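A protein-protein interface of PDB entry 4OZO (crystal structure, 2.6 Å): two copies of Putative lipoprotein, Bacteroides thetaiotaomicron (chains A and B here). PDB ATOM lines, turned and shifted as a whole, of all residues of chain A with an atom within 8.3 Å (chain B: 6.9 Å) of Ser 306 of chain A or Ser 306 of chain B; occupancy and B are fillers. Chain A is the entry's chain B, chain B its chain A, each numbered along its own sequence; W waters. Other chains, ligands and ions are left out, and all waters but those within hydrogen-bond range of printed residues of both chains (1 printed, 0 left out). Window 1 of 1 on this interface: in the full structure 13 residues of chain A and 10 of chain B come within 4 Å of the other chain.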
ATOM      1  N   GLN A  58     -26.635  -5.104  18.242  1.00  0.00           N
ATOM      2  CA  GLN A  58     -26.552  -6.183  19.210  1.00  0.00           C
ATOM      3  C   GLN A  58     -25.990  -5.641  20.520  1.00  0.00           C
ATOM      4  O   GLN A  58     -26.359  -6.111  21.595  1.00  0.00           O
ATOM      5  CB  GLN A  58     -25.700  -7.340  18.658  1.00  0.00           C
ATOM      6  CG  GLN A  58     -25.746  -8.633  19.460  1.00  0.00           C
ATOM      7  CD  GLN A  58     -24.609  -8.760  20.465  1.00  0.00           C
ATOM      8  OE1 GLN A  58     -23.642  -8.001  20.426  1.00  0.00           O
ATOM      9  NE2 GLN A  58     -24.723  -9.725  21.376  1.00  0.00           N
ATOM     10  N   GLN A  61     -28.879  -3.685  22.157  1.00  0.00           N
ATOM     11  CA  GLN A  61     -29.778  -4.678  22.725  1.00  0.00           C
ATOM     12  C   GLN A  61     -29.283  -5.055  24.123  1.00  0.00           C
ATOM     13  O   GLN A  61     -30.052  -5.056  25.082  1.00  0.00           O
ATOM     14  CB  GLN A  61     -29.887  -5.921  21.816  1.00  0.00           C
ATOM     15  CG  GLN A  61     -30.959  -5.828  20.717  1.00  0.00           C
ATOM     16  CD  GLN A  61     -30.592  -6.577  19.411  1.00  0.00           C
ATOM     17  OE1 GLN A  61     -30.418  -7.803  19.393  1.00  0.00           O
ATOM     18  NE2 GLN A  61     -30.493  -5.829  18.314  1.00  0.00           N
ATOM     19  N   THR A  62     -27.991  -5.333  24.235  1.00  0.00           N
ATOM     20  CA  THR A  62     -27.404  -5.734  25.508  1.00  0.00           C
ATOM     21  C   THR A  62     -27.581  -4.654  26.573  1.00  0.00           C
ATOM     22  O   THR A  62     -27.876  -4.955  27.733  1.00  0.00           O
ATOM     23  CB  THR A  62     -25.895  -6.078  25.364  1.00  0.00           C
ATOM     24  OG1 THR A  62     -25.727  -7.216  24.510  1.00  0.00           O
ATOM     25  CG2 THR A  62     -25.268  -6.380  26.715  1.00  0.00           C
ATOM     26  N   ALA A  65     -31.456  -4.320  27.690  1.00  0.00           N
ATOM     27  CA  ALA A  65     -31.826  -5.330  28.670  1.00  0.00           C
ATOM     28  C   ALA A  65     -31.139  -5.080  30.001  1.00  0.00           C
ATOM     29  O   ALA A  65     -31.613  -5.503  31.046  1.00  0.00           O
ATOM     30  CB  ALA A  65     -31.490  -6.736  28.160  1.00  0.00           C
ATOM     31  N   ARG A 259     -14.909  -8.391  32.628  1.00  0.00           N
ATOM     32  CA  ARG A 259     -13.916  -9.463  32.548  1.00  0.00           C
ATOM     33  C   ARG A 259     -12.619  -9.012  33.229  1.00  0.00           C
ATOM     34  O   ARG A 259     -12.470  -7.828  33.546  1.00  0.00           O
ATOM     35  CB  ARG A 259     -13.661  -9.831  31.083  1.00  0.00           C
ATOM     36  CG  ARG A 259     -14.778 -10.635  30.414  1.00  0.00           C
ATOM     37  CD  ARG A 259     -14.767 -10.420  28.905  1.00  0.00           C
ATOM     38  NE  ARG A 259     -15.824 -11.172  28.244  1.00  0.00           N
ATOM     39  CZ  ARG A 259     -15.681 -12.417  27.813  1.00  0.00           C
ATOM     40  NH1 ARG A 259     -14.521 -13.033  27.966  1.00  0.00           N
ATOM     41  NH2 ARG A 259     -16.693 -13.049  27.233  1.00  0.00           N
ATOM     42  N   TYR A 264     -11.303  -8.001  24.732  1.00  0.00           N
ATOM     43  CA  TYR A 264     -11.855  -9.347  24.709  1.00  0.00           C
ATOM     44  C   TYR A 264     -10.823 -10.440  24.454  1.00  0.00           C
ATOM     45  O   TYR A 264     -10.027 -10.357  23.514  1.00  0.00           O
ATOM     46  CB  TYR A 264     -12.972  -9.485  23.671  1.00  0.00           C
ATOM     47  CG  TYR A 264     -13.537 -10.888  23.658  1.00  0.00           C
ATOM     48  CD1 TYR A 264     -14.552 -11.243  24.531  1.00  0.00           C
ATOM     49  CD2 TYR A 264     -13.020 -11.875  22.803  1.00  0.00           C
ATOM     50  CE1 TYR A 264     -15.059 -12.528  24.542  1.00  0.00           C
ATOM     51  CE2 TYR A 264     -13.517 -13.173  22.819  1.00  0.00           C
ATOM     52  CZ  TYR A 264     -14.536 -13.491  23.690  1.00  0.00           C
ATOM     53  OH  TYR A 264     -15.056 -14.762  23.728  1.00  0.00           O
ATOM     54  N   ASP A 269     -13.654 -16.113  28.909  1.00  0.00           N
ATOM     55  CA  ASP A 269     -15.075 -16.439  28.818  1.00  0.00           C
ATOM     56  C   ASP A 269     -15.573 -17.035  30.131  1.00  0.00           C
ATOM     57  O   ASP A 269     -16.755 -16.985  30.431  1.00  0.00           O
ATOM     58  CB  ASP A 269     -15.338 -17.428  27.684  1.00  0.00           C
ATOM     59  CG  ASP A 269     -15.227 -16.797  26.312  1.00  0.00           C
ATOM     60  OD1 ASP A 269     -15.435 -15.576  26.177  1.00  0.00           O
ATOM     61  OD2 ASP A 269     -14.937 -17.526  25.348  1.00  0.00           O
ATOM     62  N   VAL A 272     -15.995 -14.199  33.473  1.00  0.00           N
ATOM     63  CA  VAL A 272     -16.953 -13.118  33.437  1.00  0.00           C
ATOM     64  C   VAL A 272     -17.567 -12.982  34.834  1.00  0.00           C
ATOM     65  O   VAL A 272     -17.904 -13.975  35.477  1.00  0.00           O
ATOM     66  CB  VAL A 272     -18.030 -13.347  32.365  1.00  0.00           C
ATOM     67  CG1 VAL A 272     -19.183 -12.379  32.539  1.00  0.00           C
ATOM     68  CG2 VAL A 272     -17.431 -13.206  30.981  1.00  0.00           C
ATOM     69  N   ASP A 299     -16.138  -9.033  20.741  1.00  0.00           N
ATOM     70  CA  ASP A 299     -15.162 -10.040  20.338  1.00  0.00           C
ATOM     71  C   ASP A 299     -14.675  -9.868  18.899  1.00  0.00           C
ATOM     72  O   ASP A 299     -14.829  -8.802  18.296  1.00  0.00           O
ATOM     73  CB  ASP A 299     -15.679 -11.475  20.552  1.00  0.00           C
ATOM     74  CG  ASP A 299     -16.883 -11.819  19.681  1.00  0.00           C
ATOM     75  OD1 ASP A 299     -17.295 -11.005  18.824  1.00  0.00           O
ATOM     76  OD2 ASP A 299     -17.426 -12.927  19.865  1.00  0.00           O
ATOM     77  N   ARG A 301     -15.901 -11.285  16.361  1.00  0.00           N
ATOM     78  CA  ARG A 301     -17.031 -11.129  15.451  1.00  0.00           C
ATOM     79  C   ARG A 301     -17.525  -9.683  15.481  1.00  0.00           C
ATOM     80  O   ARG A 301     -18.249  -9.261  14.587  1.00  0.00           O
ATOM     81  CB  ARG A 301     -18.195 -12.038  15.827  1.00  0.00           C
ATOM     82  CG  ARG A 301     -17.944 -13.527  15.787  1.00  0.00           C
ATOM     83  CD  ARG A 301     -19.110 -14.247  16.458  1.00  0.00           C
ATOM     84  NE  ARG A 301     -19.196 -13.924  17.882  1.00  0.00           N
ATOM     85  CZ  ARG A 301     -20.203 -14.268  18.684  1.00  0.00           C
ATOM     86  NH1 ARG A 301     -21.251 -14.937  18.211  1.00  0.00           N
ATOM     87  NH2 ARG A 301     -20.169 -13.934  19.970  1.00  0.00           N
ATOM     88  N   LEU A 303     -19.055  -8.631  18.443  1.00  0.00           N
ATOM     89  CA  LEU A 303     -20.277  -8.870  19.199  1.00  0.00           C
ATOM     90  C   LEU A 303     -19.981  -9.065  20.692  1.00  0.00           C
ATOM     91  O   LEU A 303     -18.889  -9.495  21.078  1.00  0.00           O
ATOM     92  CB  LEU A 303     -21.007 -10.097  18.644  1.00  0.00           C
ATOM     93  CG  LEU A 303     -21.470 -10.039  17.183  1.00  0.00           C
ATOM     94  CD1 LEU A 303     -21.803 -11.441  16.661  1.00  0.00           C
ATOM     95  CD2 LEU A 303     -22.646  -9.075  16.991  1.00  0.00           C
ATOM     96  N   ILE A 304     -20.963  -8.745  21.527  1.00  0.00           N
ATOM     97  CA  ILE A 304     -20.847  -8.970  22.961  1.00  0.00           C
ATOM     98  C   ILE A 304     -21.135 -10.444  23.257  1.00  0.00           C
ATOM     99  O   ILE A 304     -22.151 -10.987  22.804  1.00  0.00           O
ATOM    100  CB  ILE A 304     -21.830  -8.083  23.761  1.00  0.00           C
ATOM    101  CG1 ILE A 304     -21.663  -6.604  23.384  1.00  0.00           C
ATOM    102  CG2 ILE A 304     -21.659  -8.312  25.246  1.00  0.00           C
ATOM    103  CD1 ILE A 304     -20.229  -6.129  23.321  1.00  0.00           C
ATOM    104  N   HIS A 305     -20.229 -11.085  23.995  1.00  0.00           N
ATOM    105  CA  HIS A 305     -20.370 -12.490  24.335  1.00  0.00           C
ATOM    106  C   HIS A 305     -21.629 -12.691  25.174  1.00  0.00           C
ATOM    107  O   HIS A 305     -21.897 -11.915  26.087  1.00  0.00           O
ATOM    108  CB  HIS A 305     -19.142 -12.981  25.097  1.00  0.00           C
ATOM    109  CG  HIS A 305     -19.141 -14.456  25.352  1.00  0.00           C
ATOM    110  ND1 HIS A 305     -19.837 -15.033  26.393  1.00  0.00           N
ATOM    111  CD2 HIS A 305     -18.537 -15.475  24.693  1.00  0.00           C
ATOM    112  CE1 HIS A 305     -19.659 -16.343  26.366  1.00  0.00           C
ATOM    113  NE2 HIS A 305     -18.874 -16.636  25.343  1.00  0.00           N
ATOM    114  N   SER A 306     -22.399 -13.729  24.876  1.00  0.00           N
ATOM    115  CA  SER A 306     -23.717 -13.851  25.481  1.00  0.00           C
ATOM    116  C   SER A 306     -23.688 -14.007  27.015  1.00  0.00           C
ATOM    117  O   SER A 306     -24.673 -13.700  27.694  1.00  0.00           O
ATOM    118  CB  SER A 306     -24.546 -14.940  24.785  1.00  0.00           C
ATOM    119  OG  SER A 306     -24.272 -16.213  25.310  1.00  0.00           O
ATOM    120  N   THR A 307     -22.559 -14.438  27.564  1.00  0.00           N
ATOM    121  CA  THR A 307     -22.450 -14.514  29.014  1.00  0.00           C
ATOM    122  C   THR A 307     -22.388 -13.114  29.637  1.00  0.00           C
ATOM    123  O   THR A 307     -22.955 -12.861  30.696  1.00  0.00           O
ATOM    124  CB  THR A 307     -21.261 -15.391  29.466  1.00  0.00           C
ATOM    125  OG1 THR A 307     -21.543 -16.768  29.164  1.00  0.00           O
ATOM    126  CG2 THR A 307     -21.031 -15.247  30.978  1.00  0.00           C
ATOM    127  N   ASP A 308     -21.698 -12.209  28.959  1.00  0.00           N
ATOM    128  CA  ASP A 308     -21.587 -10.828  29.383  1.00  0.00           C
ATOM    129  C   ASP A 308     -22.979 -10.187  29.388  1.00  0.00           C
ATOM    130  O   ASP A 308     -23.394  -9.554  30.378  1.00  0.00           O
ATOM    131  CB  ASP A 308     -20.670 -10.066  28.413  1.00  0.00           C
ATOM    132  CG  ASP A 308     -19.302 -10.735  28.227  1.00  0.00           C
ATOM    133  OD1 ASP A 308     -19.208 -11.988  28.223  1.00  0.00           O
ATOM    134  OD2 ASP A 308     -18.310  -9.998  28.079  1.00  0.00           O
ATOM    135  N   SER A 309     -23.695 -10.355  28.274  1.00  0.00           N
ATOM    136  CA  SER A 309     -25.057  -9.847  28.132  1.00  0.00           C
ATOM    137  C   SER A 309     -25.993 -10.342  29.235  1.00  0.00           C
ATOM    138  O   SER A 309     -26.688  -9.549  29.874  1.00  0.00           O
ATOM    139  CB  SER A 309     -25.632 -10.254  26.787  1.00  0.00           C
ATOM    140  OG  SER A 309     -24.912  -9.654  25.738  1.00  0.00           O
ATOM    141  N   LEU A 310     -26.006 -11.653  29.440  1.00  0.00           N
ATOM    142  CA  LEU A 310     -26.932 -12.284  30.363  1.00  0.00           C
ATOM    143  C   LEU A 310     -26.718 -11.759  31.767  1.00  0.00           C
ATOM    144  O   LEU A 310     -27.668 -11.309  32.436  1.00  0.00           O
ATOM    145  CB  LEU A 310     -26.755 -13.802  30.362  1.00  0.00           C
ATOM    146  CG  LEU A 310     -27.659 -14.482  31.386  1.00  0.00           C
ATOM    147  CD1 LEU A 310     -29.124 -14.258  31.039  1.00  0.00           C
ATOM    148  CD2 LEU A 310     -27.355 -15.960  31.505  1.00  0.00           C
ATOM    149  N   HIS A 311     -25.468 -11.805  32.216  1.00  0.00           N
ATOM    150  CA  HIS A 311     -25.170 -11.386  33.578  1.00  0.00           C
ATOM    151  C   HIS A 311     -25.613  -9.964  33.804  1.00  0.00           C
ATOM    152  O   HIS A 311     -26.237  -9.677  34.809  1.00  0.00           O
ATOM    153  CB  HIS A 311     -23.696 -11.581  33.920  1.00  0.00           C
ATOM    154  CG  HIS A 311     -23.321 -13.018  34.094  1.00  0.00           C
ATOM    155  ND1 HIS A 311     -22.140 -13.419  34.683  1.00  0.00           N
ATOM    156  CD2 HIS A 311     -23.982 -14.153  33.762  1.00  0.00           C
ATOM    157  CE1 HIS A 311     -22.086 -14.740  34.697  1.00  0.00           C
ATOM    158  NE2 HIS A 311     -23.194 -15.209  34.150  1.00  0.00           N
ATOM    159  N   ALA A 312     -25.330  -9.085  32.852  1.00  0.00           N
ATOM    160  CA  ALA A 312     -25.745  -7.696  32.980  1.00  0.00           C
ATOM    161  C   ALA A 312     -27.265  -7.614  33.032  1.00  0.00           C
ATOM    162  O   ALA A 312     -27.833  -6.807  33.774  1.00  0.00           O
ATOM    163  CB  ALA A 312     -25.207  -6.864  31.845  1.00  0.00           C
ATOM    164  N   ALA A 313     -27.932  -8.462  32.259  1.00  0.00           N
ATOM    165  CA  ALA A 313     -29.385  -8.388  32.203  1.00  0.00           C
ATOM    166  C   ALA A 313     -30.008  -8.852  33.526  1.00  0.00           C
ATOM    167  O   ALA A 313     -31.013  -8.309  33.978  1.00  0.00           O
ATOM    168  CB  ALA A 313     -29.925  -9.172  31.017  1.00  0.00           C
ATOM    169  N   LEU A 314     -29.382  -9.838  34.156  1.00  0.00           N
ATOM    170  CA  LEU A 314     -29.896 -10.371  35.404  1.00  0.00           C
ATOM    171  C   LEU A 314     -29.618  -9.399  36.551  1.00  0.00           C
ATOM    172  O   LEU A 314     -30.379  -9.336  37.520  1.00  0.00           O
ATOM    173  CB  LEU A 314     -29.318 -11.761  35.680  1.00  0.00           C
ATOM    174  CG  LEU A 314     -29.835 -12.887  34.762  1.00  0.00           C
ATOM    175  CD1 LEU A 314     -29.174 -14.224  35.063  1.00  0.00           C
ATOM    176  CD2 LEU A 314     -31.355 -13.017  34.820  1.00  0.00           C
ATOM    177  N   GLN B  58     -21.193 -23.663  27.890  1.00  0.00           N
ATOM    178  CA  GLN B  58     -22.054 -22.492  27.913  1.00  0.00           C
ATOM    179  C   GLN B  58     -23.538 -22.888  27.754  1.00  0.00           C
ATOM    180  O   GLN B  58     -24.427 -22.262  28.355  1.00  0.00           O
ATOM    181  CB  GLN B  58     -21.598 -21.464  26.869  1.00  0.00           C
ATOM    182  CG  GLN B  58     -22.347 -20.152  26.908  1.00  0.00           C
ATOM    183  CD  GLN B  58     -23.450 -20.085  25.874  1.00  0.00           C
ATOM    184  OE1 GLN B  58     -23.587 -20.983  25.034  1.00  0.00           O
ATOM    185  NE2 GLN B  58     -24.244 -19.021  25.921  1.00  0.00           N
ATOM    186  N   THR B  62     -26.658 -22.404  30.611  1.00  0.00           N
ATOM    187  CA  THR B  62     -27.989 -21.912  30.272  1.00  0.00           C
ATOM    188  C   THR B  62     -29.042 -22.811  30.920  1.00  0.00           C
ATOM    189  O   THR B  62     -29.989 -22.337  31.548  1.00  0.00           O
ATOM    190  CB  THR B  62     -28.210 -21.859  28.743  1.00  0.00           C
ATOM    191  OG1 THR B  62     -27.328 -20.891  28.162  1.00  0.00           O
ATOM    192  CG2 THR B  62     -29.664 -21.495  28.386  1.00  0.00           C
ATOM    193  N   ARG B 259     -37.769 -20.191  19.494  1.00  0.00           N
ATOM    194  CA  ARG B 259     -37.762 -19.328  18.314  1.00  0.00           C
ATOM    195  C   ARG B 259     -38.812 -19.812  17.309  1.00  0.00           C
ATOM    196  O   ARG B 259     -39.386 -20.902  17.479  1.00  0.00           O
ATOM    197  CB  ARG B 259     -36.358 -19.300  17.697  1.00  0.00           C
ATOM    198  CG  ARG B 259     -35.425 -18.340  18.401  1.00  0.00           C
ATOM    199  CD  ARG B 259     -33.974 -18.765  18.333  1.00  0.00           C
ATOM    200  NE  ARG B 259     -33.124 -17.782  18.997  1.00  0.00           N
ATOM    201  CZ  ARG B 259     -32.467 -16.814  18.366  1.00  0.00           C
ATOM    202  NH1 ARG B 259     -32.538 -16.719  17.039  1.00  0.00           N
ATOM    203  NH2 ARG B 259     -31.727 -15.950  19.063  1.00  0.00           N
ATOM    204  N   LEU B 303     -22.699 -20.983  20.465  1.00  0.00           N
ATOM    205  CA  LEU B 303     -23.173 -20.483  21.740  1.00  0.00           C
ATOM    206  C   LEU B 303     -24.687 -20.391  21.718  1.00  0.00           C
ATOM    207  O   LEU B 303     -25.290 -20.254  20.653  1.00  0.00           O
ATOM    208  CB  LEU B 303     -22.623 -19.077  21.986  1.00  0.00           C
ATOM    209  CG  LEU B 303     -21.145 -18.848  22.312  1.00  0.00           C
ATOM    210  CD1 LEU B 303     -20.890 -17.365  22.579  1.00  0.00           C
ATOM    211  CD2 LEU B 303     -20.728 -19.711  23.497  1.00  0.00           C
ATOM    212  N   ILE B 304     -25.296 -20.440  22.902  1.00  0.00           N
ATOM    213  CA  ILE B 304     -26.708 -20.139  23.039  1.00  0.00           C
ATOM    214  C   ILE B 304     -26.873 -18.620  23.184  1.00  0.00           C
ATOM    215  O   ILE B 304     -26.245 -17.994  24.046  1.00  0.00           O
ATOM    216  CB  ILE B 304     -27.324 -20.868  24.262  1.00  0.00           C
ATOM    217  CG1 ILE B 304     -27.078 -22.380  24.181  1.00  0.00           C
ATOM    218  CG2 ILE B 304     -28.803 -20.570  24.364  1.00  0.00           C
ATOM    219  CD1 ILE B 304     -27.648 -23.073  22.909  1.00  0.00           C
ATOM    220  N   HIS B 305     -27.701 -18.034  22.322  1.00  0.00           N
ATOM    221  CA  HIS B 305     -27.992 -16.602  22.339  1.00  0.00           C
ATOM    222  C   HIS B 305     -28.534 -16.168  23.704  1.00  0.00           C
ATOM    223  O   HIS B 305     -29.265 -16.921  24.361  1.00  0.00           O
ATOM    224  CB  HIS B 305     -29.009 -16.294  21.244  1.00  0.00           C
ATOM    225  CG  HIS B 305     -29.186 -14.836  20.961  1.00  0.00           C
ATOM    226  ND1 HIS B 305     -29.865 -13.987  21.809  1.00  0.00           N
ATOM    227  CD2 HIS B 305     -28.798 -14.083  19.905  1.00  0.00           C
ATOM    228  CE1 HIS B 305     -29.876 -12.772  21.295  1.00  0.00           C
ATOM    229  NE2 HIS B 305     -29.242 -12.804  20.137  1.00  0.00           N
ATOM    230  N   SER B 306     -28.189 -14.952  24.126  1.00  0.00           N
ATOM    231  CA  SER B 306     -28.475 -14.497  25.492  1.00  0.00           C
ATOM    232  C   SER B 306     -29.925 -14.112  25.742  1.00  0.00           C
ATOM    233  O   SER B 306     -30.384 -14.176  26.874  1.00  0.00           O
ATOM    234  CB  SER B 306     -27.559 -13.342  25.886  1.00  0.00           C
ATOM    235  OG  SER B 306     -27.617 -12.310  24.922  1.00  0.00           O
ATOM    236  N   THR B 307     -30.640 -13.704  24.700  1.00  0.00           N
ATOM    237  CA  THR B 307     -32.063 -13.459  24.842  1.00  0.00           C
ATOM    238  C   THR B 307     -32.754 -14.765  25.213  1.00  0.00           C
ATOM    239  O   THR B 307     -33.579 -14.809  26.129  1.00  0.00           O
ATOM    240  CB  THR B 307     -32.704 -12.922  23.554  1.00  0.00           C
ATOM    241  OG1 THR B 307     -32.187 -11.619  23.252  1.00  0.00           O
ATOM    242  CG2 THR B 307     -34.219 -12.825  23.723  1.00  0.00           C
ATOM    243  N   ASP B 308     -32.403 -15.823  24.489  1.00  0.00           N
ATOM    244  CA  ASP B 308     -32.904 -17.156  24.756  1.00  0.00           C
ATOM    245  C   ASP B 308     -32.616 -17.508  26.214  1.00  0.00           C
ATOM    246  O   ASP B 308     -33.499 -17.960  26.952  1.00  0.00           O
ATOM    247  CB  ASP B 308     -32.220 -18.194  23.845  1.00  0.00           C
ATOM    248  CG  ASP B 308     -32.343 -17.869  22.359  1.00  0.00           C
ATOM    249  OD1 ASP B 308     -32.478 -16.692  21.980  1.00  0.00           O
ATOM    250  OD2 ASP B 308     -32.283 -18.809  21.544  1.00  0.00           O
ATOM    251  N   SER B 309     -31.365 -17.310  26.614  1.00  0.00           N
ATOM    252  CA  SER B 309     -30.957 -17.529  27.996  1.00  0.00           C
ATOM    253  C   SER B 309     -31.816 -16.739  28.977  1.00  0.00           C
ATOM    254  O   SER B 309     -32.405 -17.290  29.904  1.00  0.00           O
ATOM    255  CB  SER B 309     -29.506 -17.095  28.176  1.00  0.00           C
ATOM    256  OG  SER B 309     -28.651 -17.934  27.425  1.00  0.00           O
ATOM    257  N   LEU B 310     -31.865 -15.435  28.768  1.00  0.00           N
ATOM    258  CA  LEU B 310     -32.523 -14.559  29.698  1.00  0.00           C
ATOM    259  C   LEU B 310     -33.970 -14.998  29.919  1.00  0.00           C
ATOM    260  O   LEU B 310     -34.429 -15.109  31.058  1.00  0.00           O
ATOM    261  CB  LEU B 310     -32.465 -13.120  29.181  1.00  0.00           C
ATOM    262  CG  LEU B 310     -33.170 -12.106  30.077  1.00  0.00           C
ATOM    263  CD1 LEU B 310     -32.541 -12.132  31.437  1.00  0.00           C
ATOM    264  CD2 LEU B 310     -33.094 -10.741  29.455  1.00  0.00           C
ATOM    265  N   HIS B 311     -34.678 -15.264  28.829  1.00  0.00           N
ATOM    266  CA  HIS B 311     -36.098 -15.550  28.928  1.00  0.00           C
ATOM    267  C   HIS B 311     -36.346 -16.852  29.672  1.00  0.00           C
ATOM    268  O   HIS B 311     -37.211 -16.907  30.546  1.00  0.00           O
ATOM    269  CB  HIS B 311     -36.767 -15.531  27.555  1.00  0.00           C
ATOM    270  CG  HIS B 311     -36.795 -14.172  26.923  1.00  0.00           C
ATOM    271  ND1 HIS B 311     -37.484 -13.904  25.757  1.00  0.00           N
ATOM    272  CD2 HIS B 311     -36.215 -13.003  27.295  1.00  0.00           C
ATOM    273  CE1 HIS B 311     -37.322 -12.632  25.436  1.00  0.00           C
ATOM    274  NE2 HIS B 311     -36.556 -12.062  26.353  1.00  0.00           N
ATOM    275  N   ALA B 312     -35.569 -17.882  29.351  1.00  0.00           N
ATOM    276  CA  ALA B 312     -35.607 -19.121  30.110  1.00  0.00           C
ATOM    277  C   ALA B 312     -35.274 -18.884  31.594  1.00  0.00           C
ATOM    278  O   ALA B 312     -35.959 -19.398  32.491  1.00  0.00           O
ATOM    279  CB  ALA B 312     -34.658 -20.148  29.508  1.00  0.00           C
HETATM  280  O   HOH W   1     -24.762 -11.498  23.664  1.00  0.00           O
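His 305 of chain A touches Leu 303 of chain B, but with the chains exchanged Leu 303 of chain A does not touch His 305 of chain B (8.2 Å).
Ser 306 of chain B touches its own counterpart, Ser 306 of chain A.
Ser 309 of chain A touches Ser 306 of chain B, but with the chains exchanged Ser 306 of chain A does not touch Ser 309 of chain B (5.2 Å).
Leu 310 of chain B touches its own counterpart, Leu 310 of chain A.
Of the 8 pairs that touch across the chains among the printed residues, 2 have their exchanged pair printed and touching as well.
Water W1 lies within hydrogen-bond range of OG of Ser 309 of chain A, O of Ile 304 of chain A, NE2 of Gln 58 of chain A, OG of Ser 306 of chain B and N of Ser 306 of chain A.
Among the printed residues, pairs that only touch across the chains: Ser 309 of chain A with Ser 306 of chain B, Ser 306 of chain A with Ser 306 of chain B, His 305 of chain A with Leu 303 of chain B, Leu 310 of chain A with Leu 310 of chain B, Leu 314 of chain A with Leu 310 of chain B and Ala 313 of chain A with Leu 310 of chain B.
O of Ile 304 of chain B sits at hydrogen-bond distance from OG of Ser 306 of chain A (2.9 Å).
The side-chain amide nitrogen (NE2) of Gln 58 of chain B lies within hydrogen-bond range of the side-chain hydroxyl (OG) of Ser 306 of chain A, 2.9 Å away.
Printed residues of chain B that touch a printed residue of chain A: Gln 58, Leu 303, Ile 304, Ser 306 and Leu 310.
Hydrophobic or aromatic side chains of chain B within 4 Å of the printed part of chain A: Leu 303 and Leu 310.
Printed residues of chain A that touch a printed residue of chain B: His 305, Ser 306, Ser 309, Leu 310, Ala 313 and Leu 314.
Hydrophobic or aromatic side chains of chain A within 4 Å of the printed part of chain B: His 305, Leu 310, Ala 313 and Leu 314.
Along chain A the printed residues that touch a printed residue of chain B span positions 305 to 314.
Of chain B, only Gln 58 (2.9 Å), Ile 304 (2.9 Å) and Ser 306 (3.4 Å) come within 4 Å of Ser 306 of chain A.
Ser 306 of chain B touches just these residues of chain A: Ser 306 (3.4 Å) and Ser 309 (3.4 Å).
Of the printed residues of chain A, Gln 58 of chain B touches Ser 306.
Printed residues of chain A within 4 Å of Leu 303 of chain B: His 305.
Asp 308 of chain A touches none of the printed residues of chain B.
Tyr 264 of chain A touches none of the printed residues of chain B.
The nearest residue of chain B that does not touch Ser 306 of chain A is His 305 of chain B (4.3 Å).
The nearest printed residue of chain A that does not touch Leu 310 of chain B is Ala 65 of chain A (4.5 Å).
N of Ile 304 of chain B lies within hydrogen-bond range of OE1 of Gln 58 of chain B, 2.8 Å away.
A ring nitrogen (ND1) of His 305 of chain A is in hydrogen-bond range of the backbone NH of Thr 307 of chain A, 3.0 Å away.
The side-chain hydroxyl (OG1) of Thr 62 of chain A sits at hydrogen-bond distance from the side-chain hydroxyl (OG) of Ser 309 of chain A, at 2.8 Å.
O of Gln 58 of chain B sits at hydrogen-bond distance from OG1 of Thr 62 of chain B (3.2 Å).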
